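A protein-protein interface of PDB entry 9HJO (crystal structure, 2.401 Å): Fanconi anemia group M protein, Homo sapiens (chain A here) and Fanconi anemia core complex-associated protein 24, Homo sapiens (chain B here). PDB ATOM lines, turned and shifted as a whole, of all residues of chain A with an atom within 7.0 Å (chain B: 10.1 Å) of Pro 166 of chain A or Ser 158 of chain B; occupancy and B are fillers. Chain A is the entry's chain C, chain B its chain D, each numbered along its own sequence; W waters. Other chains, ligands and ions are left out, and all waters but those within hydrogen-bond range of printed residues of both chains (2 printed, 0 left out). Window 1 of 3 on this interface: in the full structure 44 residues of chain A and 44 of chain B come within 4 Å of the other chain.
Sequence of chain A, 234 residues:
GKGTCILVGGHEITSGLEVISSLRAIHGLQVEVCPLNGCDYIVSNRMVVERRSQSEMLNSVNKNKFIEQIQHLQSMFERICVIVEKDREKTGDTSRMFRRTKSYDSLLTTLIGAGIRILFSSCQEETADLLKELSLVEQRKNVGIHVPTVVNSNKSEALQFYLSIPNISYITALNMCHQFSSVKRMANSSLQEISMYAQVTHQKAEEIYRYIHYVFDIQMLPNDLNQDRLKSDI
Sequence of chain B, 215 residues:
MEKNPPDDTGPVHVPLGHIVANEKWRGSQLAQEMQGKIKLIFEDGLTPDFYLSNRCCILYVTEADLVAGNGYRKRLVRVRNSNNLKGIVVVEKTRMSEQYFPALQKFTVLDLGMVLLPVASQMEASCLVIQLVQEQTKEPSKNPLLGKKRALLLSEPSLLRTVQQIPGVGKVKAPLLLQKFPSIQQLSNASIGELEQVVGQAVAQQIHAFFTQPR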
ATOM      1  N   SER A  75      29.435  14.476  14.991  1.00  0.00           N
ATOM      2  CA  SER A  75      29.561  13.467  16.027  1.00  0.00           C
ATOM      3  C   SER A  75      28.364  12.509  16.043  1.00  0.00           C
ATOM      4  O   SER A  75      28.494  11.435  16.618  1.00  0.00           O
ATOM      5  CB  SER A  75      29.769  14.084  17.375  1.00  0.00           C
ATOM      6  OG  SER A  75      28.608  14.768  17.810  1.00  0.00           O
ATOM      7  N   MET A  76      27.219  12.860  15.413  1.00  0.00           N
ATOM      8  CA  MET A  76      26.031  12.015  15.456  1.00  0.00           C
ATOM      9  C   MET A  76      25.574  11.497  14.104  1.00  0.00           C
ATOM     10  O   MET A  76      24.702  10.630  14.089  1.00  0.00           O
ATOM     11  CB  MET A  76      24.846  12.759  16.061  1.00  0.00           C
ATOM     12  CG  MET A  76      25.117  13.327  17.417  1.00  0.00           C
ATOM     13  SD  MET A  76      23.683  14.274  17.937  1.00  0.00           S
ATOM     14  CE  MET A  76      23.966  15.915  17.255  1.00  0.00           C
ATOM     15  N   TYR A 162      17.515   7.992  27.311  1.00  0.00           N
ATOM     16  CA  TYR A 162      18.350   7.651  26.174  1.00  0.00           C
ATOM     17  C   TYR A 162      18.917   8.909  25.512  1.00  0.00           C
ATOM     18  O   TYR A 162      20.078   8.918  25.102  1.00  0.00           O
ATOM     19  CB  TYR A 162      17.553   6.830  25.172  1.00  0.00           C
ATOM     20  CG  TYR A 162      17.198   5.423  25.621  1.00  0.00           C
ATOM     21  CD1 TYR A 162      18.138   4.573  26.193  1.00  0.00           C
ATOM     22  CD2 TYR A 162      15.908   4.930  25.427  1.00  0.00           C
ATOM     23  CE1 TYR A 162      17.792   3.298  26.617  1.00  0.00           C
ATOM     24  CE2 TYR A 162      15.553   3.665  25.847  1.00  0.00           C
ATOM     25  CZ  TYR A 162      16.502   2.842  26.425  1.00  0.00           C
ATOM     26  OH  TYR A 162      16.117   1.588  26.776  1.00  0.00           O
ATOM     27  N   LEU A 163      18.100   9.966  25.401  1.00  0.00           N
ATOM     28  CA  LEU A 163      18.552  11.256  24.893  1.00  0.00           C
ATOM     29  C   LEU A 163      19.702  11.827  25.730  1.00  0.00           C
ATOM     30  O   LEU A 163      20.460  12.603  25.170  1.00  0.00           O
ATOM     31  CB  LEU A 163      17.373  12.228  24.877  1.00  0.00           C
ATOM     32  CG  LEU A 163      16.350  12.010  23.761  1.00  0.00           C
ATOM     33  CD1 LEU A 163      15.107  12.820  24.082  1.00  0.00           C
ATOM     34  CD2 LEU A 163      16.919  12.347  22.387  1.00  0.00           C
ATOM     35  N   SER A 164      19.781  11.502  27.047  1.00  0.00           N
ATOM     36  CA  SER A 164      20.862  11.940  27.917  1.00  0.00           C
ATOM     37  C   SER A 164      22.197  11.286  27.570  1.00  0.00           C
ATOM     38  O   SER A 164      23.212  11.747  28.072  1.00  0.00           O
ATOM     39  CB  SER A 164      20.544  11.711  29.368  1.00  0.00           C
ATOM     40  OG  SER A 164      20.783  10.364  29.769  1.00  0.00           O
ATOM     41  N   ILE A 165      22.223  10.228  26.741  1.00  0.00           N
ATOM     42  CA  ILE A 165      23.470   9.589  26.338  1.00  0.00           C
ATOM     43  C   ILE A 165      24.234  10.518  25.400  1.00  0.00           C
ATOM     44  O   ILE A 165      23.662  10.955  24.421  1.00  0.00           O
ATOM     45  CB  ILE A 165      23.215   8.225  25.680  1.00  0.00           C
ATOM     46  CG1 ILE A 165      22.573   7.274  26.665  1.00  0.00           C
ATOM     47  CG2 ILE A 165      24.466   7.625  25.034  1.00  0.00           C
ATOM     48  CD1 ILE A 165      22.016   6.048  25.995  1.00  0.00           C
ATOM     49  N   PRO A 166      25.524  10.846  25.668  1.00  0.00           N
ATOM     50  CA  PRO A 166      26.260  11.809  24.867  1.00  0.00           C
ATOM     51  C   PRO A 166      26.397  11.440  23.401  1.00  0.00           C
ATOM     52  O   PRO A 166      26.537  10.275  23.072  1.00  0.00           O
ATOM     53  CB  PRO A 166      27.682  11.814  25.468  1.00  0.00           C
ATOM     54  CG  PRO A 166      27.408  11.450  26.896  1.00  0.00           C
ATOM     55  CD  PRO A 166      26.312  10.425  26.844  1.00  0.00           C
ATOM     56  N   ASN A 167      26.431  12.467  22.553  1.00  0.00           N
ATOM     57  CA  ASN A 167      26.681  12.309  21.138  1.00  0.00           C
ATOM     58  C   ASN A 167      25.807  11.239  20.494  1.00  0.00           C
ATOM     59  O   ASN A 167      26.318  10.552  19.623  1.00  0.00           O
ATOM     60  CB  ASN A 167      28.151  12.049  20.922  1.00  0.00           C
ATOM     61  CG  ASN A 167      28.943  13.096  21.636  1.00  0.00           C
ATOM     62  OD1 ASN A 167      29.717  12.774  22.536  1.00  0.00           O
ATOM     63  ND2 ASN A 167      28.719  14.344  21.266  1.00  0.00           N
ATOM     64  N   ILE A 168      24.507  11.151  20.846  1.00  0.00           N
ATOM     65  CA  ILE A 168      23.557  10.447  19.990  1.00  0.00           C
ATOM     66  C   ILE A 168      22.402  11.381  19.588  1.00  0.00           C
ATOM     67  O   ILE A 168      21.959  12.244  20.349  1.00  0.00           O
ATOM     68  CB  ILE A 168      23.040   9.135  20.629  1.00  0.00           C
ATOM     69  CG1 ILE A 168      22.000   9.332  21.752  1.00  0.00           C
ATOM     70  CG2 ILE A 168      24.196   8.251  21.097  1.00  0.00           C
ATOM     71  CD1 ILE A 168      21.212   8.077  22.073  1.00  0.00           C
ATOM     72  N   SER A 169      21.870  11.133  18.397  1.00  0.00           N
ATOM     73  CA  SER A 169      20.789  11.908  17.821  1.00  0.00           C
ATOM     74  C   SER A 169      19.441  11.483  18.398  1.00  0.00           C
ATOM     75  O   SER A 169      19.335  10.408  19.003  1.00  0.00           O
ATOM     76  CB  SER A 169      20.775  11.704  16.362  1.00  0.00           C
ATOM     77  OG  SER A 169      20.194  10.436  16.070  1.00  0.00           O
ATOM     78  N   LYS A 204      29.903   4.024  16.686  1.00  0.00           N
ATOM     79  CA  LYS A 204      28.904   4.718  17.485  1.00  0.00           C
ATOM     80  C   LYS A 204      28.327   3.787  18.556  1.00  0.00           C
ATOM     81  O   LYS A 204      28.097   4.227  19.687  1.00  0.00           O
ATOM     82  CB  LYS A 204      27.889   5.391  16.552  1.00  0.00           C
ATOM     83  CG  LYS A 204      26.742   6.102  17.283  1.00  0.00           C
ATOM     84  CD  LYS A 204      27.112   7.223  18.235  1.00  0.00           C
ATOM     85  CE  LYS A 204      27.741   8.320  17.429  1.00  0.00           C
ATOM     86  NZ  LYS A 204      28.048   9.448  18.299  1.00  0.00           N
ATOM     87  N   GLU A 207      30.813   3.643  21.264  1.00  0.00           N
ATOM     88  CA  GLU A 207      30.787   4.786  22.181  1.00  0.00           C
ATOM     89  C   GLU A 207      29.665   4.636  23.204  1.00  0.00           C
ATOM     90  O   GLU A 207      29.820   4.990  24.363  1.00  0.00           O
ATOM     91  CB  GLU A 207      30.528   6.177  21.616  1.00  0.00           C
ATOM     92  CG  GLU A 207      31.557   6.745  20.647  1.00  0.00           C
ATOM     93  CD  GLU A 207      30.995   7.918  19.827  1.00  0.00           C
ATOM     94  OE1 GLU A 207      30.080   8.644  20.321  1.00  0.00           O
ATOM     95  OE2 GLU A 207      31.377   8.042  18.620  1.00  0.00           O
ATOM     96  N   ILE A 208      28.516   4.129  22.764  1.00  0.00           N
ATOM     97  CA  ILE A 208      27.390   3.942  23.647  1.00  0.00           C
ATOM     98  C   ILE A 208      27.690   2.820  24.650  1.00  0.00           C
ATOM     99  O   ILE A 208      27.329   2.955  25.820  1.00  0.00           O
ATOM    100  CB  ILE A 208      26.139   3.641  22.809  1.00  0.00           C
ATOM    101  CG1 ILE A 208      25.765   4.824  21.930  1.00  0.00           C
ATOM    102  CG2 ILE A 208      24.960   3.183  23.689  1.00  0.00           C
ATOM    103  CD1 ILE A 208      24.918   4.410  20.744  1.00  0.00           C
ATOM    104  N   TYR A 211      30.049   3.872  27.311  1.00  0.00           N
ATOM    105  CA  TYR A 211      29.397   4.806  28.214  1.00  0.00           C
ATOM    106  C   TYR A 211      28.607   4.077  29.286  1.00  0.00           C
ATOM    107  O   TYR A 211      28.711   4.430  30.464  1.00  0.00           O
ATOM    108  CB  TYR A 211      28.495   5.740  27.405  1.00  0.00           C
ATOM    109  CG  TYR A 211      27.785   6.796  28.224  1.00  0.00           C
ATOM    110  CD1 TYR A 211      28.496   7.834  28.796  1.00  0.00           C
ATOM    111  CD2 TYR A 211      26.406   6.769  28.386  1.00  0.00           C
ATOM    112  CE1 TYR A 211      27.869   8.800  29.564  1.00  0.00           C
ATOM    113  CE2 TYR A 211      25.763   7.722  29.174  1.00  0.00           C
ATOM    114  CZ  TYR A 211      26.499   8.751  29.756  1.00  0.00           C
ATOM    115  OH  TYR A 211      25.883   9.734  30.497  1.00  0.00           O
ATOM    116  N   LEU A 221      35.506  14.226  39.769  1.00  0.00           N
ATOM    117  CA  LEU A 221      34.739  15.469  39.815  1.00  0.00           C
ATOM    118  C   LEU A 221      35.330  16.356  40.886  1.00  0.00           C
ATOM    119  O   LEU A 221      35.955  15.799  41.770  1.00  0.00           O
ATOM    120  CB  LEU A 221      33.275  15.166  40.144  1.00  0.00           C
ATOM    121  CG  LEU A 221      32.517  14.434  39.047  1.00  0.00           C
ATOM    122  CD1 LEU A 221      31.173  13.982  39.551  1.00  0.00           C
ATOM    123  CD2 LEU A 221      32.386  15.307  37.820  1.00  0.00           C
ATOM    124  N   LEU B 153      36.975  13.681  27.127  1.00  0.00           N
ATOM    125  CA  LEU B 153      36.137  14.025  28.312  1.00  0.00           C
ATOM    126  C   LEU B 153      35.911  12.802  29.229  1.00  0.00           C
ATOM    127  O   LEU B 153      35.794  11.641  28.813  1.00  0.00           O
ATOM    128  CB  LEU B 153      34.790  14.667  27.934  1.00  0.00           C
ATOM    129  CG  LEU B 153      34.791  16.015  27.188  1.00  0.00           C
ATOM    130  CD1 LEU B 153      33.334  16.432  26.939  1.00  0.00           C
ATOM    131  CD2 LEU B 153      35.562  17.174  27.865  1.00  0.00           C
ATOM    132  N   LEU B 154      35.896  13.112  30.530  1.00  0.00           N
ATOM    133  CA  LEU B 154      35.270  12.319  31.566  1.00  0.00           C
ATOM    134  C   LEU B 154      33.774  12.199  31.279  1.00  0.00           C
ATOM    135  O   LEU B 154      33.112  13.167  30.942  1.00  0.00           O
ATOM    136  CB  LEU B 154      35.426  13.058  32.893  1.00  0.00           C
ATOM    137  CG  LEU B 154      36.830  13.304  33.429  1.00  0.00           C
ATOM    138  CD1 LEU B 154      36.655  14.243  34.604  1.00  0.00           C
ATOM    139  CD2 LEU B 154      37.551  12.023  33.810  1.00  0.00           C
ATOM    140  N   SER B 155      33.243  11.003  31.482  1.00  0.00           N
ATOM    141  CA  SER B 155      31.830  10.728  31.392  1.00  0.00           C
ATOM    142  C   SER B 155      31.131  11.029  32.712  1.00  0.00           C
ATOM    143  O   SER B 155      29.913  11.108  32.724  1.00  0.00           O
ATOM    144  CB  SER B 155      31.621   9.317  30.974  1.00  0.00           C
ATOM    145  OG  SER B 155      32.289   9.016  29.762  1.00  0.00           O
ATOM    146  N   GLU B 156      31.872  11.205  33.815  1.00  0.00           N
ATOM    147  CA  GLU B 156      31.272  11.421  35.125  1.00  0.00           C
ATOM    148  C   GLU B 156      30.132  12.448  35.056  1.00  0.00           C
ATOM    149  O   GLU B 156      29.015  12.110  35.434  1.00  0.00           O
ATOM    150  CB  GLU B 156      32.320  11.813  36.165  1.00  0.00           C
ATOM    151  CG  GLU B 156      33.011  10.642  36.841  1.00  0.00           C
ATOM    152  CD  GLU B 156      34.053   9.900  36.039  1.00  0.00           C
ATOM    153  OE1 GLU B 156      34.423  10.271  34.886  1.00  0.00           O
ATOM    154  OE2 GLU B 156      34.532   8.915  36.685  1.00  0.00           O
ATOM    155  N   PRO B 157      30.331  13.692  34.543  1.00  0.00           N
ATOM    156  CA  PRO B 157      29.266  14.702  34.527  1.00  0.00           C
ATOM    157  C   PRO B 157      28.020  14.265  33.766  1.00  0.00           C
ATOM    158  O   PRO B 157      26.919  14.403  34.286  1.00  0.00           O
ATOM    159  CB  PRO B 157      29.885  15.969  33.922  1.00  0.00           C
ATOM    160  CG  PRO B 157      31.380  15.736  34.056  1.00  0.00           C
ATOM    161  CD  PRO B 157      31.599  14.234  34.010  1.00  0.00           C
ATOM    162  N   SER B 158      28.219  13.704  32.574  1.00  0.00           N
ATOM    163  CA  SER B 158      27.135  13.144  31.785  1.00  0.00           C
ATOM    164  C   SER B 158      26.398  12.040  32.535  1.00  0.00           C
ATOM    165  O   SER B 158      25.181  11.950  32.448  1.00  0.00           O
ATOM    166  CB  SER B 158      27.651  12.629  30.470  1.00  0.00           C
ATOM    167  OG  SER B 158      28.210  13.719  29.756  1.00  0.00           O
ATOM    168  N   LEU B 159      27.136  11.161  33.233  1.00  0.00           N
ATOM    169  CA  LEU B 159      26.516  10.021  33.891  1.00  0.00           C
ATOM    170  C   LEU B 159      25.615  10.501  35.030  1.00  0.00           C
ATOM    171  O   LEU B 159      24.524   9.943  35.191  1.00  0.00           O
ATOM    172  CB  LEU B 159      27.589   9.053  34.353  1.00  0.00           C
ATOM    173  CG  LEU B 159      28.297   8.267  33.249  1.00  0.00           C
ATOM    174  CD1 LEU B 159      29.563   7.663  33.877  1.00  0.00           C
ATOM    175  CD2 LEU B 159      27.473   7.181  32.624  1.00  0.00           C
ATOM    176  N   LEU B 160      26.032  11.576  35.737  1.00  0.00           N
ATOM    177  CA  LEU B 160      25.211  12.205  36.768  1.00  0.00           C
ATOM    178  C   LEU B 160      23.870  12.615  36.171  1.00  0.00           C
ATOM    179  O   LEU B 160      22.843  12.272  36.757  1.00  0.00           O
ATOM    180  CB  LEU B 160      25.888  13.386  37.476  1.00  0.00           C
ATOM    181  CG  LEU B 160      27.049  13.041  38.420  1.00  0.00           C
ATOM    182  CD1 LEU B 160      27.815  14.238  38.912  1.00  0.00           C
ATOM    183  CD2 LEU B 160      26.564  12.199  39.574  1.00  0.00           C
ATOM    184  N   ARG B 161      23.913  13.296  35.005  1.00  0.00           N
ATOM    185  CA  ARG B 161      22.736  13.779  34.305  1.00  0.00           C
ATOM    186  C   ARG B 161      21.880  12.631  33.783  1.00  0.00           C
ATOM    187  O   ARG B 161      20.661  12.741  33.809  1.00  0.00           O
ATOM    188  CB  ARG B 161      23.067  14.658  33.102  1.00  0.00           C
ATOM    189  CG  ARG B 161      23.749  15.948  33.511  1.00  0.00           C
ATOM    190  CD  ARG B 161      23.976  16.854  32.298  1.00  0.00           C
ATOM    191  NE  ARG B 161      25.351  17.379  32.291  1.00  0.00           N
ATOM    192  CZ  ARG B 161      26.317  17.042  31.434  1.00  0.00           C
ATOM    193  NH1 ARG B 161      26.053  16.346  30.331  1.00  0.00           N
ATOM    194  NH2 ARG B 161      27.549  17.444  31.673  1.00  0.00           N
ATOM    195  N   THR B 162      22.501  11.563  33.278  1.00  0.00           N
ATOM    196  CA  THR B 162      21.742  10.408  32.812  1.00  0.00           C
ATOM    197  C   THR B 162      20.945   9.800  33.974  1.00  0.00           C
ATOM    198  O   THR B 162      19.734   9.608  33.882  1.00  0.00           O
ATOM    199  CB  THR B 162      22.668   9.385  32.154  1.00  0.00           C
ATOM    200  OG1 THR B 162      23.256   9.975  30.992  1.00  0.00           O
ATOM    201  CG2 THR B 162      21.943   8.090  31.800  1.00  0.00           C
ATOM    202  N   VAL B 163      21.643   9.536  35.084  1.00  0.00           N
ATOM    203  CA  VAL B 163      21.048   8.970  36.282  1.00  0.00           C
ATOM    204  C   VAL B 163      19.977   9.894  36.871  1.00  0.00           C
ATOM    205  O   VAL B 163      18.991   9.404  37.398  1.00  0.00           O
ATOM    206  CB  VAL B 163      22.205   8.629  37.245  1.00  0.00           C
ATOM    207  CG1 VAL B 163      21.746   8.439  38.685  1.00  0.00           C
ATOM    208  CG2 VAL B 163      22.958   7.400  36.736  1.00  0.00           C
ATOM    209  N   GLN B 164      20.131  11.212  36.755  1.00  0.00           N
ATOM    210  CA  GLN B 164      19.084  12.148  37.152  1.00  0.00           C
ATOM    211  C   GLN B 164      17.798  12.078  36.303  1.00  0.00           C
ATOM    212  O   GLN B 164      16.781  12.610  36.748  1.00  0.00           O
ATOM    213  CB  GLN B 164      19.650  13.566  37.204  1.00  0.00           C
ATOM    214  CG  GLN B 164      20.505  13.792  38.441  1.00  0.00           C
ATOM    215  CD  GLN B 164      21.175  15.143  38.472  1.00  0.00           C
ATOM    216  OE1 GLN B 164      20.575  16.160  38.817  1.00  0.00           O
ATOM    217  NE2 GLN B 164      22.458  15.151  38.170  1.00  0.00           N
ATOM    218  N   GLN B 165      17.822  11.437  35.121  1.00  0.00           N
ATOM    219  CA  GLN B 165      16.612  11.153  34.365  1.00  0.00           C
ATOM    220  C   GLN B 165      15.783  10.031  34.990  1.00  0.00           C
ATOM    221  O   GLN B 165      14.612   9.880  34.615  1.00  0.00           O
ATOM    222  CB  GLN B 165      16.872  10.724  32.925  1.00  0.00           C
ATOM    223  CG  GLN B 165      17.682  11.724  32.111  1.00  0.00           C
ATOM    224  CD  GLN B 165      17.286  13.152  32.387  1.00  0.00           C
ATOM    225  OE1 GLN B 165      16.130  13.521  32.208  1.00  0.00           O
ATOM    226  NE2 GLN B 165      18.208  13.925  32.937  1.00  0.00           N
ATOM    227  N   ILE B 166      16.361   9.251  35.922  1.00  0.00           N
ATOM    228  CA  ILE B 166      15.607   8.211  36.610  1.00  0.00           C
ATOM    229  C   ILE B 166      14.677   8.926  37.592  1.00  0.00           C
ATOM    230  O   ILE B 166      15.155   9.762  38.351  1.00  0.00           O
ATOM    231  CB  ILE B 166      16.531   7.195  37.301  1.00  0.00           C
ATOM    232  CG1 ILE B 166      17.492   6.545  36.309  1.00  0.00           C
ATOM    233  CG2 ILE B 166      15.720   6.145  38.061  1.00  0.00           C
ATOM    234  CD1 ILE B 166      18.714   5.917  36.949  1.00  0.00           C
ATOM    235  N   ALA B 174      21.842  10.996  42.792  1.00  0.00           N
ATOM    236  CA  ALA B 174      22.580  10.511  41.631  1.00  0.00           C
ATOM    237  C   ALA B 174      23.998  10.061  41.999  1.00  0.00           C
ATOM    238  O   ALA B 174      24.340   8.910  41.727  1.00  0.00           O
ATOM    239  CB  ALA B 174      22.603  11.540  40.527  1.00  0.00           C
ATOM    240  N   LEU B 178      25.803   6.136  41.929  1.00  0.00           N
ATOM    241  CA  LEU B 178      26.947   5.820  41.089  1.00  0.00           C
ATOM    242  C   LEU B 178      28.188   5.498  41.931  1.00  0.00           C
ATOM    243  O   LEU B 178      29.122   4.911  41.414  1.00  0.00           O
ATOM    244  CB  LEU B 178      27.200   6.932  40.078  1.00  0.00           C
ATOM    245  CG  LEU B 178      26.219   6.998  38.907  1.00  0.00           C
ATOM    246  CD1 LEU B 178      26.444   8.259  38.123  1.00  0.00           C
ATOM    247  CD2 LEU B 178      26.350   5.815  37.964  1.00  0.00           C
ATOM    248  N   ILE B 184      26.169   2.350  34.438  1.00  0.00           N
ATOM    249  CA  ILE B 184      24.738   2.339  34.150  1.00  0.00           C
ATOM    250  C   ILE B 184      24.285   0.881  34.194  1.00  0.00           C
ATOM    251  O   ILE B 184      23.274   0.614  34.823  1.00  0.00           O
ATOM    252  CB  ILE B 184      24.363   3.046  32.828  1.00  0.00           C
ATOM    253  CG1 ILE B 184      24.685   4.528  32.839  1.00  0.00           C
ATOM    254  CG2 ILE B 184      22.893   2.821  32.456  1.00  0.00           C
ATOM    255  CD1 ILE B 184      23.893   5.339  33.841  1.00  0.00           C
HETATM  256  O   HOH W   1      28.357   3.879  33.243  1.00  0.00           O
HETATM  257  O   HOH W   2      23.921  12.815  30.231  1.00  0.00           O
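Among the printed residues, merely in contact across the chains: Leu 221 of chain A with Leu 160 of chain B (3.4 Å), Pro 166 of chain A with Ser 158 of chain B (3.7 Å), Leu 221 of chain A with Glu 156 of chain B (3.9 Å), Leu 221 of chain A with Pro 157 of chain B (3.9 Å) and Ser 164 of chain A with Gln 165 of chain B (3.96 Å).
The side-chain hydroxyl (OG) of Ser 164 of chain A lies within hydrogen-bond range of the side-chain hydroxyl (OG1) of Thr 162 of chain B (2.8 Å).
The backbone carbonyl oxygen (O) of Ser 158 of chain B sits at hydrogen-bond distance from the side-chain hydroxyl (OH) of Tyr 211 of chain A (3.0 Å).
The backbone NH of Leu 159 of chain B sits at hydrogen-bond distance from the side-chain hydroxyl of Tyr 211 of chain A.
OH of Tyr 211 of chain A lies within hydrogen-bond range of OG1 of Thr 162 of chain B, at 2.7 Å.
Pro 166 of chain A touches just one residue of chain B: Ser 158.
Ser 158 of chain B touches just these residues of chain A: Pro 166 (3.7 Å) and Tyr 211 (3.0 Å).
Ser 164 of chain A touches just these residues of chain B: Thr 162 (2.8 Å) and Gln 165 (3.96 Å).
No residue of chain B comes within 4 Å of Asn 167 of chain A.
No residue of chain B comes within 4 Å of Ile 168 of chain A.
Of the printed residues of chain A, Glu 156 of chain B touches Leu 221.
Of the printed residues of chain B, Tyr 211 of chain A touches Ser 158, Leu 159 and Thr 162.
Ile 184 of chain B touches none of the printed residues of chain A.
Ser 75 of chain A touches none of the printed residues of chain B.
The side-chain hydroxyl (OG) of Ser 158 of chain B is in hydrogen-bond range of the guanidinium group (NH1) of Arg 161 of chain B (3.4 Å).
OG1 of Thr 162 of chain B is in hydrogen-bond range of O of Ser 158 of chain B, 3.1 Å away.
NE2 of Gln 164 of chain B lies within hydrogen-bond range of O of Leu 160 of chain B (3.2 Å).
The backbone carbonyl oxygen (O) of Arg 161 of chain B is in hydrogen-bond range of the side-chain amide nitrogen (NE2) of Gln 165 of chain B (2.9 Å).
Printed residues of chain B that touch a printed residue of chain A: Glu 156, Pro 157, Ser 158, Leu 159, Leu 160, Thr 162 and Gln 165.
Hydrophobic or aromatic side chains of chain B that line the printed part of chain A: Pro 157, Leu 159 and Leu 160.
Along chain B the printed residues that touch a printed residue of chain A span positions 156 to 165.
Printed residues of chain A that touch a printed residue of chain B: Ser 164, Pro 166, Tyr 211 and Leu 221.
Hydrophobic or aromatic side chains of chain A within 4 Å of the printed part of chain B: Pro 166, Tyr 211 and Leu 221.
Along chain A the printed residues that touch a printed residue of chain B span positions 164 to 221.
Among the printed residues, no Asp or Glu carboxylate lies within 4 Å of a Lys or Arg side-chain nitrogen of the other chain.
Water W2 lies within hydrogen-bond range of the backbone carbonyl oxygen of Ser 164 of chain A (2.5 Å), the backbone carbonyl oxygen of Ser 158 of chain B (2.7 Å) and the side-chain hydroxyl of Thr 162 of chain B (3.0 Å).
Water W1 lies within hydrogen-bond range of O of Tyr 211 of chain A (2.9 Å) and N of Ile 184 of chain B (2.9 Å).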
